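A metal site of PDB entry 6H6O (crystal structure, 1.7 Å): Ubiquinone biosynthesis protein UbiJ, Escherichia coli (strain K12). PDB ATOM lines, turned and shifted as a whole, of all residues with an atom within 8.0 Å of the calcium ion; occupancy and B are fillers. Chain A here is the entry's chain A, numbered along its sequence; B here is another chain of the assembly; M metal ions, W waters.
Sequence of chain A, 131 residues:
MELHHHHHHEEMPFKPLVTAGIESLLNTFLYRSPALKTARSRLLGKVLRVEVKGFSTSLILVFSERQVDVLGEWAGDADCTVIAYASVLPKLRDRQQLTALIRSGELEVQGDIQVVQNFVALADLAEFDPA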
ATOM      1  N   THR A  28     -11.535   0.734  24.118  1.00  0.00           N
ATOM      2  CA  THR A  28     -12.259   1.979  24.433  1.00  0.00           C
ATOM      3  C   THR A  28     -13.640   1.992  23.777  1.00  0.00           C
ATOM      4  O   THR A  28     -14.616   2.447  24.392  1.00  0.00           O
ATOM      5  CB  THR A  28     -11.419   3.206  24.029  1.00  0.00           C
ATOM      6  OG1 THR A  28     -10.116   3.090  24.617  1.00  0.00           O
ATOM      7  CG2 THR A  28     -12.073   4.533  24.439  1.00  0.00           C
ATOM      8  N   PHE A  29     -13.747   1.480  22.548  1.00  0.00           N
ATOM      9  CA  PHE A  29     -15.000   1.492  21.794  1.00  0.00           C
ATOM     10  C   PHE A  29     -16.036   0.455  22.267  1.00  0.00           C
ATOM     11  O   PHE A  29     -17.232   0.774  22.388  1.00  0.00           O
ATOM     12  CB  PHE A  29     -14.697   1.337  20.287  1.00  0.00           C
ATOM     13  CG  PHE A  29     -15.874   1.426  19.349  1.00  0.00           C
ATOM     14  CD1 PHE A  29     -16.634   2.595  19.258  1.00  0.00           C
ATOM     15  CD2 PHE A  29     -16.217   0.357  18.528  1.00  0.00           C
ATOM     16  CE1 PHE A  29     -17.715   2.689  18.372  1.00  0.00           C
ATOM     17  CE2 PHE A  29     -17.311   0.437  17.657  1.00  0.00           C
ATOM     18  CZ  PHE A  29     -18.043   1.603  17.579  1.00  0.00           C
ATOM     19  N   LEU A  30     -15.567  -0.763  22.572  1.00  0.00           N
ATOM     20  CA  LEU A  30     -16.414  -1.910  22.894  1.00  0.00           C
ATOM     21  C   LEU A  30     -16.524  -2.305  24.349  1.00  0.00           C
ATOM     22  O   LEU A  30     -17.570  -2.810  24.738  1.00  0.00           O
ATOM     23  CB  LEU A  30     -15.956  -3.138  22.085  1.00  0.00           C
ATOM     24  CG  LEU A  30     -15.887  -3.002  20.555  1.00  0.00           C
ATOM     25  CD1 LEU A  30     -15.278  -4.241  19.939  1.00  0.00           C
ATOM     26  CD2 LEU A  30     -17.287  -2.716  19.909  1.00  0.00           C
ATOM     27  N   ARG A  32     -15.574  -0.232  27.258  1.00  0.00           N
ATOM     28  CA  ARG A  32     -15.671   0.823  28.268  1.00  0.00           C
ATOM     29  C   ARG A  32     -17.090   0.919  28.873  1.00  0.00           C
ATOM     30  O   ARG A  32     -17.211   1.156  30.073  1.00  0.00           O
ATOM     31  CB  ARG A  32     -15.260   2.174  27.651  1.00  0.00           C
ATOM     32  CG  ARG A  32     -15.207   3.359  28.593  1.00  0.00           C
ATOM     33  CD  ARG A  32     -14.643   4.572  27.884  1.00  0.00           C
ATOM     34  NE  ARG A  32     -14.645   5.762  28.739  1.00  0.00           N
ATOM     35  CZ  ARG A  32     -13.623   6.135  29.512  1.00  0.00           C
ATOM     36  NH1 ARG A  32     -13.718   7.228  30.262  1.00  0.00           N
ATOM     37  NH2 ARG A  32     -12.509   5.406  29.549  1.00  0.00           N
ATOM     38  N   SER A  33     -18.139   0.723  28.059  1.00  0.00           N
ATOM     39  CA  SER A  33     -19.502   0.872  28.554  1.00  0.00           C
ATOM     40  C   SER A  33     -20.079  -0.386  29.199  1.00  0.00           C
ATOM     41  O   SER A  33     -20.232  -1.416  28.530  1.00  0.00           O
ATOM     42  CB  SER A  33     -20.421   1.386  27.470  1.00  0.00           C
ATOM     43  OG  SER A  33     -21.744   1.442  27.983  1.00  0.00           O
ATOM     44  N   LEU A  36     -23.145  -2.510  27.422  1.00  0.00           N
ATOM     45  CA  LEU A  36     -22.910  -3.520  26.370  1.00  0.00           C
ATOM     46  C   LEU A  36     -22.602  -4.940  26.870  1.00  0.00           C
ATOM     47  O   LEU A  36     -22.370  -5.844  26.052  1.00  0.00           O
ATOM     48  CB  LEU A  36     -21.785  -3.046  25.445  1.00  0.00           C
ATOM     49  CG  LEU A  36     -21.971  -1.702  24.751  1.00  0.00           C
ATOM     50  CD1 LEU A  36     -20.753  -1.367  23.926  1.00  0.00           C
ATOM     51  CD2 LEU A  36     -23.216  -1.700  23.868  1.00  0.00           C
ATOM     52  N   LEU A 122     -22.333  -6.308  18.120  1.00  0.00           N
ATOM     53  CA  LEU A 122     -21.710  -5.576  19.230  1.00  0.00           C
ATOM     54  C   LEU A 122     -21.254  -4.189  18.785  1.00  0.00           C
ATOM     55  O   LEU A 122     -21.574  -3.206  19.476  1.00  0.00           O
ATOM     56  CB  LEU A 122     -20.537  -6.373  19.872  1.00  0.00           C
ATOM     57  CG  LEU A 122     -19.641  -5.635  20.896  1.00  0.00           C
ATOM     58  CD1 LEU A 122     -20.446  -5.116  22.093  1.00  0.00           C
ATOM     59  CD2 LEU A 122     -18.475  -6.519  21.346  1.00  0.00           C
ATOM     60  N   ALA A 123     -20.554  -4.073  17.633  1.00  0.00           N
ATOM     61  CA  ALA A 123     -20.105  -2.772  17.114  1.00  0.00           C
ATOM     62  C   ALA A 123     -21.316  -1.845  16.834  1.00  0.00           C
ATOM     63  O   ALA A 123     -21.258  -0.639  17.134  1.00  0.00           O
ATOM     64  CB  ALA A 123     -19.272  -2.955  15.860  1.00  0.00           C
ATOM     65  N   ASP A 124     -22.418  -2.431  16.293  1.00  0.00           N
ATOM     66  CA  ASP A 124     -23.659  -1.696  16.012  1.00  0.00           C
ATOM     67  C   ASP A 124     -24.244  -1.130  17.330  1.00  0.00           C
ATOM     68  O   ASP A 124     -24.561   0.049  17.403  1.00  0.00           O
ATOM     69  CB  ASP A 124     -24.676  -2.614  15.306  1.00  0.00           C
ATOM     70  CG  ASP A 124     -25.840  -1.877  14.647  1.00  0.00           C
ATOM     71  OD1 ASP A 124     -25.796  -0.640  14.554  1.00  0.00           O
ATOM     72  OD2 ASP A 124     -26.804  -2.561  14.205  1.00  0.00           O
ATOM     73  N   LEU A 125     -24.275  -1.966  18.388  1.00  0.00           N
ATOM     74  CA  LEU A 125     -24.796  -1.529  19.675  1.00  0.00           C
ATOM     75  C   LEU A 125     -23.859  -0.539  20.360  1.00  0.00           C
ATOM     76  O   LEU A 125     -24.337   0.332  21.086  1.00  0.00           O
ATOM     77  CB  LEU A 125     -25.095  -2.735  20.568  1.00  0.00           C
ATOM     78  CG  LEU A 125     -26.319  -3.577  20.118  1.00  0.00           C
ATOM     79  CD1 LEU A 125     -26.398  -4.884  20.859  1.00  0.00           C
ATOM     80  CD2 LEU A 125     -27.646  -2.805  20.300  1.00  0.00           C
ATOM     81  N   ALA A 126     -22.536  -0.643  20.109  1.00  0.00           N
ATOM     82  CA  ALA A 126     -21.553   0.275  20.667  1.00  0.00           C
ATOM     83  C   ALA A 126     -21.695   1.694  20.110  1.00  0.00           C
ATOM     84  O   ALA A 126     -21.366   2.685  20.785  1.00  0.00           O
ATOM     85  CB  ALA A 126     -20.123  -0.255  20.477  1.00  0.00           C
ATOM     86  N   GLU A 127     -22.204   1.792  18.883  1.00  0.00           N
ATOM     87  CA  GLU A 127     -22.490   3.071  18.231  1.00  0.00           C
ATOM     88  C   GLU A 127     -23.819   3.622  18.789  1.00  0.00           C
ATOM     89  O   GLU A 127     -23.944   4.832  19.014  1.00  0.00           O
ATOM     90  CB  GLU A 127     -22.591   2.876  16.732  1.00  0.00           C
ATOM     91  CG  GLU A 127     -22.440   4.148  15.927  1.00  0.00           C
ATOM     92  CD  GLU A 127     -22.740   4.017  14.438  1.00  0.00           C
ATOM     93  OE1 GLU A 127     -23.333   2.994  14.030  1.00  0.00           O
ATOM     94  OE2 GLU A 127     -22.422   4.972  13.693  1.00  0.00           O
ATOM     95  N   PHE A 128     -24.816   2.725  19.021  1.00  0.00           N
ATOM     96  CA  PHE A 128     -26.126   3.095  19.570  1.00  0.00           C
ATOM     97  C   PHE A 128     -25.972   3.693  20.976  1.00  0.00           C
ATOM     98  O   PHE A 128     -26.612   4.683  21.321  1.00  0.00           O
ATOM     99  CB  PHE A 128     -27.077   1.875  19.596  1.00  0.00           C
ATOM    100  CG  PHE A 128     -28.138   1.894  20.692  1.00  0.00           C
ATOM    101  CD1 PHE A 128     -29.261   2.713  20.574  1.00  0.00           C
ATOM    102  CD2 PHE A 128     -27.988   1.126  21.838  1.00  0.00           C
ATOM    103  CE1 PHE A 128     -30.214   2.758  21.596  1.00  0.00           C
ATOM    104  CE2 PHE A 128     -28.940   1.182  22.870  1.00  0.00           C
ATOM    105  CZ  PHE A 128     -30.045   1.995  22.736  1.00  0.00           C
ATOM    106  N   ASP A 129     -25.193   3.006  21.808  1.00  0.00           N
ATOM    107  CA  ASP A 129     -24.969   3.395  23.180  1.00  0.00           C
ATOM    108  C   ASP A 129     -24.056   4.647  23.217  1.00  0.00           C
ATOM    109  O   ASP A 129     -22.914   4.567  22.792  1.00  0.00           O
ATOM    110  CB  ASP A 129     -24.372   2.208  23.958  1.00  0.00           C
ATOM    111  CG  ASP A 129     -23.940   2.577  25.344  1.00  0.00           C
ATOM    112  OD1 ASP A 129     -24.624   3.374  25.969  1.00  0.00           O
ATOM    113  OD2 ASP A 129     -22.913   2.060  25.783  1.00  0.00           O
ATOM    114  N   PRO A 130     -24.552   5.799  23.728  1.00  0.00           N
ATOM    115  CA  PRO A 130     -23.726   7.039  23.701  1.00  0.00           C
ATOM    116  C   PRO A 130     -22.524   7.079  24.648  1.00  0.00           C
ATOM    117  O   PRO A 130     -21.707   7.995  24.531  1.00  0.00           O
ATOM    118  CB  PRO A 130     -24.735   8.151  23.991  1.00  0.00           C
ATOM    119  CG  PRO A 130     -25.829   7.485  24.755  1.00  0.00           C
ATOM    120  CD  PRO A 130     -25.896   6.057  24.258  1.00  0.00           C
ATOM    121  N   ALA A 131     -22.365   6.093  25.559  1.00  0.00           N
ATOM    122  CA  ALA A 131     -21.217   6.037  26.472  1.00  0.00           C
ATOM    123  C   ALA A 131     -19.919   5.712  25.719  1.00  0.00           C
ATOM    124  O   ALA A 131     -19.936   5.081  24.652  1.00  0.00           O
ATOM    125  CB  ALA A 131     -21.465   5.002  27.552  1.00  0.00           C
ATOM    126  N   PHE B  14     -16.322   8.036  17.350  1.00  0.00           N
ATOM    127  CA  PHE B  14     -15.353   7.075  16.823  1.00  0.00           C
ATOM    128  C   PHE B  14     -14.129   7.743  16.142  1.00  0.00           C
ATOM    129  O   PHE B  14     -13.018   7.316  16.425  1.00  0.00           O
ATOM    130  CB  PHE B  14     -16.034   6.052  15.892  1.00  0.00           C
ATOM    131  CG  PHE B  14     -15.190   4.826  15.587  1.00  0.00           C
ATOM    132  CD1 PHE B  14     -14.833   3.932  16.589  1.00  0.00           C
ATOM    133  CD2 PHE B  14     -14.780   4.557  14.288  1.00  0.00           C
ATOM    134  CE1 PHE B  14     -14.052   2.814  16.304  1.00  0.00           C
ATOM    135  CE2 PHE B  14     -14.018   3.424  14.001  1.00  0.00           C
ATOM    136  CZ  PHE B  14     -13.653   2.563  15.018  1.00  0.00           C
ATOM    137  N   LEU B  17     -11.264   8.947  18.385  1.00  0.00           N
ATOM    138  CA  LEU B  17     -10.551   7.774  18.929  1.00  0.00           C
ATOM    139  C   LEU B  17      -9.573   7.199  17.921  1.00  0.00           C
ATOM    140  O   LEU B  17      -8.438   6.842  18.284  1.00  0.00           O
ATOM    141  CB  LEU B  17     -11.542   6.686  19.402  1.00  0.00           C
ATOM    142  CG  LEU B  17     -12.269   6.958  20.705  1.00  0.00           C
ATOM    143  CD1 LEU B  17     -13.286   5.861  20.986  1.00  0.00           C
ATOM    144  CD2 LEU B  17     -11.290   7.018  21.856  1.00  0.00           C
HETATM  145 CA    CA M   1     -20.676   3.971  22.462  1.00  0.00          CA
HETATM  146  O   HOH W   1     -18.419   3.208  22.367  1.00  0.00           O
HETATM  147  O   HOH W   2     -20.850   2.230  24.006  1.00  0.00           O
HETATM  148  O   HOH W   3     -20.474   5.740  21.012  1.00  0.00           O
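The side-chain hydroxyl (OG) of Ser 33 sits at hydrogen-bond distance from the side-chain carboxylate (OD2) of Asp 129 (2.6 Å).
The nearest printed residue that does not touch the calcium ion is Pro 130 (4.2 Å).
The calcium ion is bound by the backbone carbonyl oxygen (O) of Ala 126 (2.2 Å), water W3 (2.3 Å), water W2 (2.3 Å), the backbone carbonyl oxygen (O) of Asp 129 (2.3 Å), water W1 (2.4 Å) and the backbone carbonyl oxygen (O) of Ala 131 (2.6 Å).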
